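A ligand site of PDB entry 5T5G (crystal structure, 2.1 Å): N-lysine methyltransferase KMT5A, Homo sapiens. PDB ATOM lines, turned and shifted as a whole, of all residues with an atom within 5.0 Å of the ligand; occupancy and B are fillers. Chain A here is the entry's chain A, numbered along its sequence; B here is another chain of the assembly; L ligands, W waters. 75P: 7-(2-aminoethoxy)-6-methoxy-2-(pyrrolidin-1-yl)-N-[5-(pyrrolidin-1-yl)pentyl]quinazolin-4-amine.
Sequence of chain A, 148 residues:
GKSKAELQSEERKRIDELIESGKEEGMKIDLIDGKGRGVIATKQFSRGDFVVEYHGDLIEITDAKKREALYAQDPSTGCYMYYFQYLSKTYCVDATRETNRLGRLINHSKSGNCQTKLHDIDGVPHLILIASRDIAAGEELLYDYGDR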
ATOM      1  N   ARG A  37     -13.351 -24.613  11.881  1.00  0.00           N
ATOM      2  CA  ARG A  37     -13.833 -23.779  13.000  1.00  0.00           C
ATOM      3  C   ARG A  37     -14.967 -24.440  13.824  1.00  0.00           C
ATOM      4  O   ARG A  37     -15.507 -23.823  14.747  1.00  0.00           O
ATOM      5  CB  ARG A  37     -14.172 -22.366  12.484  1.00  0.00           C
ATOM      6  CG  ARG A  37     -15.068 -22.329  11.254  1.00  0.00           C
ATOM      7  CD  ARG A  37     -16.473 -22.851  11.522  1.00  0.00           C
ATOM      8  NE  ARG A  37     -17.050 -22.144  12.665  1.00  0.00           N
ATOM      9  CZ  ARG A  37     -18.077 -22.561  13.428  1.00  0.00           C
ATOM     10  NH1 ARG A  37     -18.734 -23.729  13.211  1.00  0.00           N
ATOM     11  NH2 ARG A  37     -18.458 -21.778  14.426  1.00  0.00           N
ATOM     12  N   TYR A  54     -12.148 -36.770  23.103  1.00  0.00           N
ATOM     13  CA  TYR A  54     -11.306 -35.567  23.174  1.00  0.00           C
ATOM     14  C   TYR A  54      -9.880 -36.061  23.302  1.00  0.00           C
ATOM     15  O   TYR A  54      -9.418 -36.357  24.389  1.00  0.00           O
ATOM     16  CB  TYR A  54     -11.664 -34.714  24.359  1.00  0.00           C
ATOM     17  CG  TYR A  54     -10.847 -33.433  24.503  1.00  0.00           C
ATOM     18  CD1 TYR A  54     -11.061 -32.351  23.664  1.00  0.00           C
ATOM     19  CD2 TYR A  54      -9.923 -33.282  25.510  1.00  0.00           C
ATOM     20  CE1 TYR A  54     -10.356 -31.150  23.827  1.00  0.00           C
ATOM     21  CE2 TYR A  54      -9.224 -32.099  25.681  1.00  0.00           C
ATOM     22  CZ  TYR A  54      -9.446 -31.027  24.836  1.00  0.00           C
ATOM     23  OH  TYR A  54      -8.756 -29.854  25.002  1.00  0.00           O
ATOM     24  N   GLY A  78      -4.144 -21.492  22.738  1.00  0.00           N
ATOM     25  CA  GLY A  78      -5.364 -21.846  23.388  1.00  0.00           C
ATOM     26  C   GLY A  78      -5.129 -22.674  24.649  1.00  0.00           C
ATOM     27  O   GLY A  78      -4.062 -23.288  24.841  1.00  0.00           O
ATOM     28  N   CYS A  79      -6.156 -22.672  25.501  1.00  0.00           N
ATOM     29  CA  CYS A  79      -6.195 -23.476  26.717  1.00  0.00           C
ATOM     30  C   CYS A  79      -6.912 -24.795  26.399  1.00  0.00           C
ATOM     31  O   CYS A  79      -8.168 -24.868  26.410  1.00  0.00           O
ATOM     32  CB  CYS A  79      -6.920 -22.668  27.798  1.00  0.00           C
ATOM     33  SG  CYS A  79      -6.337 -20.937  27.826  1.00  0.00           S
ATOM     34  N   TYR A  80      -6.143 -25.808  26.082  1.00  0.00           N
ATOM     35  CA  TYR A  80      -6.679 -27.108  25.662  1.00  0.00           C
ATOM     36  C   TYR A  80      -6.443 -28.167  26.709  1.00  0.00           C
ATOM     37  O   TYR A  80      -6.628 -29.353  26.449  1.00  0.00           O
ATOM     38  CB  TYR A  80      -6.050 -27.550  24.345  1.00  0.00           C
ATOM     39  CG  TYR A  80      -6.538 -26.799  23.147  1.00  0.00           C
ATOM     40  CD1 TYR A  80      -7.683 -27.193  22.479  1.00  0.00           C
ATOM     41  CD2 TYR A  80      -5.822 -25.692  22.655  1.00  0.00           C
ATOM     42  CE1 TYR A  80      -8.135 -26.515  21.352  1.00  0.00           C
ATOM     43  CE2 TYR A  80      -6.253 -25.002  21.549  1.00  0.00           C
ATOM     44  CZ  TYR A  80      -7.416 -25.414  20.908  1.00  0.00           C
ATOM     45  OH  TYR A  80      -7.821 -24.726  19.820  1.00  0.00           O
ATOM     46  N   MET A  81      -5.986 -27.754  27.892  1.00  0.00           N
ATOM     47  CA  MET A  81      -5.596 -28.711  28.923  1.00  0.00           C
ATOM     48  C   MET A  81      -6.820 -28.964  29.792  1.00  0.00           C
ATOM     49  O   MET A  81      -7.329 -28.016  30.399  1.00  0.00           O
ATOM     50  CB  MET A  81      -4.416 -28.145  29.735  1.00  0.00           C
ATOM     51  CG  MET A  81      -3.188 -27.888  28.849  1.00  0.00           C
ATOM     52  SD  MET A  81      -1.696 -27.364  29.718  1.00  0.00           S
ATOM     53  CE  MET A  81      -1.203 -28.887  30.522  1.00  0.00           C
ATOM     54  N   TYR A  82      -7.300 -30.207  29.828  1.00  0.00           N
ATOM     55  CA  TYR A  82      -8.502 -30.566  30.604  1.00  0.00           C
ATOM     56  C   TYR A  82      -8.038 -31.462  31.748  1.00  0.00           C
ATOM     57  O   TYR A  82      -7.572 -32.564  31.510  1.00  0.00           O
ATOM     58  CB  TYR A  82      -9.528 -31.295  29.719  1.00  0.00           C
ATOM     59  CG  TYR A  82     -10.799 -31.703  30.453  1.00  0.00           C
ATOM     60  CD1 TYR A  82     -11.878 -30.799  30.628  1.00  0.00           C
ATOM     61  CD2 TYR A  82     -10.915 -32.972  31.011  1.00  0.00           C
ATOM     62  CE1 TYR A  82     -13.032 -31.196  31.309  1.00  0.00           C
ATOM     63  CE2 TYR A  82     -12.077 -33.364  31.696  1.00  0.00           C
ATOM     64  CZ  TYR A  82     -13.135 -32.470  31.832  1.00  0.00           C
ATOM     65  OH  TYR A  82     -14.261 -32.842  32.513  1.00  0.00           O
ATOM     66  N   GLY A 103     -12.240 -34.163  17.871  1.00  0.00           N
ATOM     67  CA  GLY A 103     -12.763 -33.896  19.191  1.00  0.00           C
ATOM     68  C   GLY A 103     -12.439 -32.493  19.686  1.00  0.00           C
ATOM     69  O   GLY A 103     -13.301 -31.781  20.225  1.00  0.00           O
ATOM     70  N   ARG A 104     -11.196 -32.096  19.456  1.00  0.00           N
ATOM     71  CA  ARG A 104     -10.694 -30.795  19.941  1.00  0.00           C
ATOM     72  C   ARG A 104     -11.208 -29.557  19.123  1.00  0.00           C
ATOM     73  O   ARG A 104     -10.887 -28.451  19.466  1.00  0.00           O
ATOM     74  CB  ARG A 104      -9.147 -30.830  19.973  1.00  0.00           C
ATOM     75  CG  ARG A 104      -8.475 -31.018  18.630  1.00  0.00           C
ATOM     76  CD  ARG A 104      -6.972 -31.243  18.770  1.00  0.00           C
ATOM     77  NE  ARG A 104      -6.309 -30.034  19.231  1.00  0.00           N
ATOM     78  CZ  ARG A 104      -6.083 -28.955  18.484  1.00  0.00           C
ATOM     79  NH1 ARG A 104      -6.417 -28.915  17.191  1.00  0.00           N
ATOM     80  NH2 ARG A 104      -5.486 -27.912  19.041  1.00  0.00           N
ATOM     81  N   LEU A 105     -11.938 -29.795  18.041  1.00  0.00           N
ATOM     82  CA  LEU A 105     -12.465 -28.714  17.176  1.00  0.00           C
ATOM     83  C   LEU A 105     -13.950 -28.417  17.407  1.00  0.00           C
ATOM     84  O   LEU A 105     -14.478 -27.459  16.849  1.00  0.00           O
ATOM     85  CB  LEU A 105     -12.226 -29.059  15.704  1.00  0.00           C
ATOM     86  CG  LEU A 105     -10.752 -29.357  15.304  1.00  0.00           C
ATOM     87  CD1 LEU A 105     -10.686 -29.699  13.813  1.00  0.00           C
ATOM     88  CD2 LEU A 105      -9.776 -28.216  15.596  1.00  0.00           C
ATOM     89  N   ILE A 106     -14.614 -29.246  18.231  1.00  0.00           N
ATOM     90  CA  ILE A 106     -16.024 -29.112  18.564  1.00  0.00           C
ATOM     91  C   ILE A 106     -16.176 -27.931  19.514  1.00  0.00           C
ATOM     92  O   ILE A 106     -15.556 -27.882  20.590  1.00  0.00           O
ATOM     93  CB  ILE A 106     -16.560 -30.394  19.281  1.00  0.00           C
ATOM     94  CG1 ILE A 106     -16.541 -31.566  18.305  1.00  0.00           C
ATOM     95  CG2 ILE A 106     -17.947 -30.200  19.867  1.00  0.00           C
ATOM     96  CD1 ILE A 106     -17.045 -32.871  18.798  1.00  0.00           C
ATOM     97  N   ASN A 107     -16.983 -26.982  19.121  1.00  0.00           N
ATOM     98  CA  ASN A 107     -17.232 -25.828  19.972  1.00  0.00           C
ATOM     99  C   ASN A 107     -18.079 -26.143  21.180  1.00  0.00           C
ATOM    100  O   ASN A 107     -18.830 -27.125  21.216  1.00  0.00           O
ATOM    101  CB  ASN A 107     -17.916 -24.729  19.176  1.00  0.00           C
ATOM    102  CG  ASN A 107     -17.008 -24.144  18.129  1.00  0.00           C
ATOM    103  OD1 ASN A 107     -15.893 -23.751  18.429  1.00  0.00           O
ATOM    104  ND2 ASN A 107     -17.471 -24.062  16.905  1.00  0.00           N
ATOM    105  N   THR A 116     -19.537 -34.628  28.306  1.00  0.00           N
ATOM    106  CA  THR A 116     -18.360 -35.381  28.670  1.00  0.00           C
ATOM    107  C   THR A 116     -18.699 -36.618  29.496  1.00  0.00           C
ATOM    108  O   THR A 116     -19.639 -36.627  30.270  1.00  0.00           O
ATOM    109  CB  THR A 116     -17.354 -34.533  29.468  1.00  0.00           C
ATOM    110  OG1 THR A 116     -17.989 -34.018  30.641  1.00  0.00           O
ATOM    111  CG2 THR A 116     -16.845 -33.414  28.613  1.00  0.00           C
ATOM    112  N   LEU A 127     -11.327 -39.453  27.885  1.00  0.00           N
ATOM    113  CA  LEU A 127     -12.417 -38.459  27.932  1.00  0.00           C
ATOM    114  C   LEU A 127     -13.089 -38.443  26.559  1.00  0.00           C
ATOM    115  O   LEU A 127     -12.439 -38.160  25.557  1.00  0.00           O
ATOM    116  CB  LEU A 127     -11.875 -37.095  28.290  1.00  0.00           C
ATOM    117  CG  LEU A 127     -12.929 -36.053  28.658  1.00  0.00           C
ATOM    118  CD1 LEU A 127     -13.692 -36.320  29.947  1.00  0.00           C
ATOM    119  CD2 LEU A 127     -12.205 -34.725  28.728  1.00  0.00           C
ATOM    120  N   LEU A 129     -16.939 -37.791  24.283  1.00  0.00           N
ATOM    121  CA  LEU A 129     -18.128 -37.034  24.168  1.00  0.00           C
ATOM    122  C   LEU A 129     -19.205 -37.996  23.704  1.00  0.00           C
ATOM    123  O   LEU A 129     -18.991 -38.736  22.742  1.00  0.00           O
ATOM    124  CB  LEU A 129     -17.908 -35.931  23.145  1.00  0.00           C
ATOM    125  CG  LEU A 129     -17.051 -34.721  23.558  1.00  0.00           C
ATOM    126  CD1 LEU A 129     -16.929 -33.801  22.366  1.00  0.00           C
ATOM    127  CD2 LEU A 129     -17.700 -33.949  24.698  1.00  0.00           C
ATOM    128  N   TYR A 143     -20.403 -29.115  22.586  1.00  0.00           N
ATOM    129  CA  TYR A 143     -20.219 -29.783  23.879  1.00  0.00           C
ATOM    130  C   TYR A 143     -20.511 -28.868  25.109  1.00  0.00           C
ATOM    131  O   TYR A 143     -20.369 -27.678  25.035  1.00  0.00           O
ATOM    132  CB  TYR A 143     -18.808 -30.374  23.968  1.00  0.00           C
ATOM    133  CG  TYR A 143     -17.740 -29.404  24.451  1.00  0.00           C
ATOM    134  CD1 TYR A 143     -17.470 -29.276  25.786  1.00  0.00           C
ATOM    135  CD2 TYR A 143     -17.041 -28.629  23.568  1.00  0.00           C
ATOM    136  CE1 TYR A 143     -16.513 -28.393  26.238  1.00  0.00           C
ATOM    137  CE2 TYR A 143     -16.075 -27.756  24.001  1.00  0.00           C
ATOM    138  CZ  TYR A 143     -15.811 -27.646  25.343  1.00  0.00           C
ATOM    139  OH  TYR A 143     -14.847 -26.767  25.789  1.00  0.00           O
ATOM    140  N   TYR A 145     -20.052 -29.691  29.770  1.00  0.00           N
ATOM    141  CA  TYR A 145     -19.424 -30.618  30.753  1.00  0.00           C
ATOM    142  C   TYR A 145     -20.402 -31.509  31.561  1.00  0.00           C
ATOM    143  O   TYR A 145     -21.598 -31.208  31.683  1.00  0.00           O
ATOM    144  CB  TYR A 145     -18.556 -29.813  31.713  1.00  0.00           C
ATOM    145  CG  TYR A 145     -17.428 -29.074  31.011  1.00  0.00           C
ATOM    146  CD1 TYR A 145     -16.240 -29.716  30.670  1.00  0.00           C
ATOM    147  CD2 TYR A 145     -17.556 -27.738  30.646  1.00  0.00           C
ATOM    148  CE1 TYR A 145     -15.193 -29.016  30.035  1.00  0.00           C
ATOM    149  CE2 TYR A 145     -16.518 -27.048  30.006  1.00  0.00           C
ATOM    150  CZ  TYR A 145     -15.329 -27.706  29.717  1.00  0.00           C
ATOM    151  OH  TYR A 145     -14.293 -27.061  29.072  1.00  0.00           O
ATOM    152  N   GLU B  68     -15.612 -23.889  35.620  1.00  0.00           N
ATOM    153  CA  GLU B  68     -15.047 -23.965  34.283  1.00  0.00           C
ATOM    154  C   GLU B  68     -16.153 -23.923  33.228  1.00  0.00           C
ATOM    155  O   GLU B  68     -16.092 -23.138  32.289  1.00  0.00           O
ATOM    156  CB  GLU B  68     -14.206 -25.234  34.118  1.00  0.00           C
ATOM    157  CG  GLU B  68     -13.238 -25.185  32.951  1.00  0.00           C
ATOM    158  CD  GLU B  68     -12.382 -26.434  32.887  1.00  0.00           C
ATOM    159  OE1 GLU B  68     -12.958 -27.517  32.699  1.00  0.00           O
ATOM    160  OE2 GLU B  68     -11.159 -26.322  33.049  1.00  0.00           O
ATOM    161  N   TYR B  71     -17.609 -20.312  32.951  1.00  0.00           N
ATOM    162  CA  TYR B  71     -16.698 -19.424  32.259  1.00  0.00           C
ATOM    163  C   TYR B  71     -16.590 -19.713  30.767  1.00  0.00           C
ATOM    164  O   TYR B  71     -16.274 -18.834  30.001  1.00  0.00           O
ATOM    165  CB  TYR B  71     -15.305 -19.507  32.858  1.00  0.00           C
ATOM    166  CG  TYR B  71     -15.191 -19.205  34.330  1.00  0.00           C
ATOM    167  CD1 TYR B  71     -16.040 -18.315  34.977  1.00  0.00           C
ATOM    168  CD2 TYR B  71     -14.160 -19.770  35.063  1.00  0.00           C
ATOM    169  CE1 TYR B  71     -15.879 -18.021  36.313  1.00  0.00           C
ATOM    170  CE2 TYR B  71     -13.989 -19.489  36.405  1.00  0.00           C
ATOM    171  CZ  TYR B  71     -14.852 -18.615  37.026  1.00  0.00           C
ATOM    172  OH  TYR B  71     -14.674 -18.351  38.353  1.00  0.00           O
ATOM    173  N   THR B  77     -13.087 -14.410  28.669  1.00  0.00           N
ATOM    174  CA  THR B  77     -12.459 -14.844  29.949  1.00  0.00           C
ATOM    175  C   THR B  77     -11.041 -15.370  29.823  1.00  0.00           C
ATOM    176  O   THR B  77     -10.761 -16.309  29.074  1.00  0.00           O
ATOM    177  CB  THR B  77     -13.254 -16.001  30.635  1.00  0.00           C
ATOM    178  OG1 THR B  77     -14.664 -15.718  30.582  1.00  0.00           O
ATOM    179  CG2 THR B  77     -12.824 -16.208  32.103  1.00  0.00           C
ATOM    180  N   GLY B  78     -10.148 -14.794  30.600  1.00  0.00           N
ATOM    181  CA  GLY B  78      -8.847 -15.357  30.796  1.00  0.00           C
ATOM    182  C   GLY B  78      -8.896 -16.696  31.525  1.00  0.00           C
ATOM    183  O   GLY B  78      -9.887 -17.034  32.200  1.00  0.00           O
ATOM    184  N   CYS B  79      -7.805 -17.445  31.360  1.00  0.00           N
ATOM    185  CA  CYS B  79      -7.597 -18.716  32.036  1.00  0.00           C
ATOM    186  C   CYS B  79      -6.786 -18.442  33.319  1.00  0.00           C
ATOM    187  O   CYS B  79      -5.537 -18.352  33.286  1.00  0.00           O
ATOM    188  CB  CYS B  79      -6.862 -19.660  31.078  1.00  0.00           C
ATOM    189  SG  CYS B  79      -7.588 -19.588  29.411  1.00  0.00           S
ATOM    190  N   MET B  81      -7.314 -20.260  36.197  1.00  0.00           N
ATOM    191  CA  MET B  81      -7.532 -21.403  37.083  1.00  0.00           C
ATOM    192  C   MET B  81      -6.218 -22.170  37.154  1.00  0.00           C
ATOM    193  O   MET B  81      -5.750 -22.650  36.117  1.00  0.00           O
ATOM    194  CB  MET B  81      -8.683 -22.266  36.550  1.00  0.00           C
ATOM    195  CG  MET B  81      -9.998 -21.477  36.478  1.00  0.00           C
ATOM    196  SD  MET B  81     -11.460 -22.427  35.992  1.00  0.00           S
ATOM    197  CE  MET B  81     -11.736 -23.402  37.486  1.00  0.00           C
HETATM  198  C4  75P L   1     -12.072 -27.573  23.665  1.00  0.00           C
HETATM  199  C5  75P L   1     -11.149 -26.899  24.522  1.00  0.00           C
HETATM  200  C6  75P L   1     -10.950 -27.503  25.823  1.00  0.00           C
HETATM  201  N1  75P L   1     -11.620 -28.596  26.177  1.00  0.00           N
HETATM  202  N3  75P L   1     -12.741 -28.700  24.049  1.00  0.00           N
HETATM  203  NBA 75P L   1     -13.311 -23.386  18.986  1.00  0.00           N
HETATM  204  CAZ 75P L   1     -12.943 -24.789  18.656  1.00  0.00           C
HETATM  205  CAY 75P L   1     -12.923 -25.636  19.895  1.00  0.00           C
HETATM  206  OAX 75P L   1     -11.908 -25.232  20.790  1.00  0.00           O
HETATM  207  CAW 75P L   1     -11.733 -25.866  21.985  1.00  0.00           C
HETATM  208  CAC 75P L   1     -10.826 -25.199  22.843  1.00  0.00           C
HETATM  209  OAB 75P L   1     -10.285 -24.055  22.302  1.00  0.00           O
HETATM  210  CAA 75P L   1      -9.286 -23.362  23.061  1.00  0.00           C
HETATM  211  CAD 75P L   1     -10.551 -25.696  24.072  1.00  0.00           C
HETATM  212  CAV 75P L   1     -12.335 -27.026  22.396  1.00  0.00           C
HETATM  213  C2  75P L   1     -12.489 -29.149  25.302  1.00  0.00           C
HETATM  214  NBB 75P L   1     -13.148 -30.252  25.700  1.00  0.00           N
HETATM  215  CBF 75P L   1     -13.024 -30.778  27.061  1.00  0.00           C
HETATM  216  CBE 75P L   1     -13.596 -32.158  26.943  1.00  0.00           C
HETATM  217  CBD 75P L   1     -14.667 -32.023  25.900  1.00  0.00           C
HETATM  218  CBC 75P L   1     -14.137 -31.007  24.928  1.00  0.00           C
HETATM  219  NAG 75P L   1     -10.021 -26.943  26.740  1.00  0.00           N
HETATM  220  CAH 75P L   1      -9.768 -27.492  28.055  1.00  0.00           C
HETATM  221  CAI 75P L   1     -10.821 -27.027  29.036  1.00  0.00           C
HETATM  222  CAJ 75P L   1     -10.556 -25.627  29.564  1.00  0.00           C
HETATM  223  CAK 75P L   1     -11.549 -24.557  29.134  1.00  0.00           C
HETATM  224  CAL 75P L   1     -10.941 -23.178  29.249  1.00  0.00           C
HETATM  225  NAM 75P L   1     -11.400 -22.400  30.446  1.00  0.00           N
HETATM  226  CAN 75P L   1     -11.479 -20.912  30.240  1.00  0.00           C
HETATM  227  CAQ 75P L   1     -10.546 -22.543  31.682  1.00  0.00           C
HETATM  228  CAP 75P L   1     -11.036 -21.417  32.557  1.00  0.00           C
HETATM  229  CAO 75P L   1     -11.371 -20.279  31.614  1.00  0.00           C
HETATM  230  O   HOH W   1     -14.128 -29.851  22.009  1.00  0.00           O
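Residues that only touch the ligand: Tyr 80 (3.3 Å), Met 81 of chain A (3.4 Å), Tyr 82 (3.7 Å), Arg 104 (3.5 Å), Leu 105 (3.6 Å), Ile 106 (3.5 Å), Thr 116 (3.7 Å), Leu 127 (3.4 Å), Leu 129 (3.8 Å), Tyr 145 (3.5 Å), Glu 68 of chain B (3.6 Å), Gly 78 of chain B (3.6 Å) and Met 81 of chain B (3.6 Å). Hydrophobic or aromatic side chains within 4 Å of the ligand: Tyr 54, Tyr 80, Tyr 82, Leu 127, Leu 129, Tyr 143 and Met 81 of chain B. Along chain A the residues within 4 Å of the ligand span positions 54 to 145.
The backbone carbonyl oxygen of Tyr 80 is in hydrogen-bond range of the side-chain hydroxyl of Tyr 54, 2.6 Å away. O of Leu 127 lies within hydrogen-bond range of N of Tyr 54. OH of Tyr 145 sits at hydrogen-bond distance from OH of Tyr 143 (3.3 Å). The side-chain amide nitrogen (ND2) of Asn 107 sits at hydrogen-bond distance from the backbone carbonyl oxygen (O) of Arg 37. The side-chain sulfur of Cys 79 of chain B is disulfide-bonded to the side-chain sulfur of Cys 79 of chain A, at 2.4 Å. The backbone NH (N) of Tyr 143 sits at hydrogen-bond distance from the backbone carbonyl oxygen (O) of Asn 107.
The side-chain hydroxyl of Tyr 143 is in hydrogen-bond range of a nitrogen (N3) of the ligand, at 3.3 Å. The side-chain amide oxygen (OD1) of Asn 107 lies within hydrogen-bond range of a nitrogen (NBA) of the ligand (2.7 Å). The backbone carbonyl oxygen of Cys 79 of chain A sits at hydrogen-bond distance from a nitrogen (NAG) of the ligand, at 2.8 Å. N1 of the ligand sits close to OH of Tyr 54 (3.3 Å).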
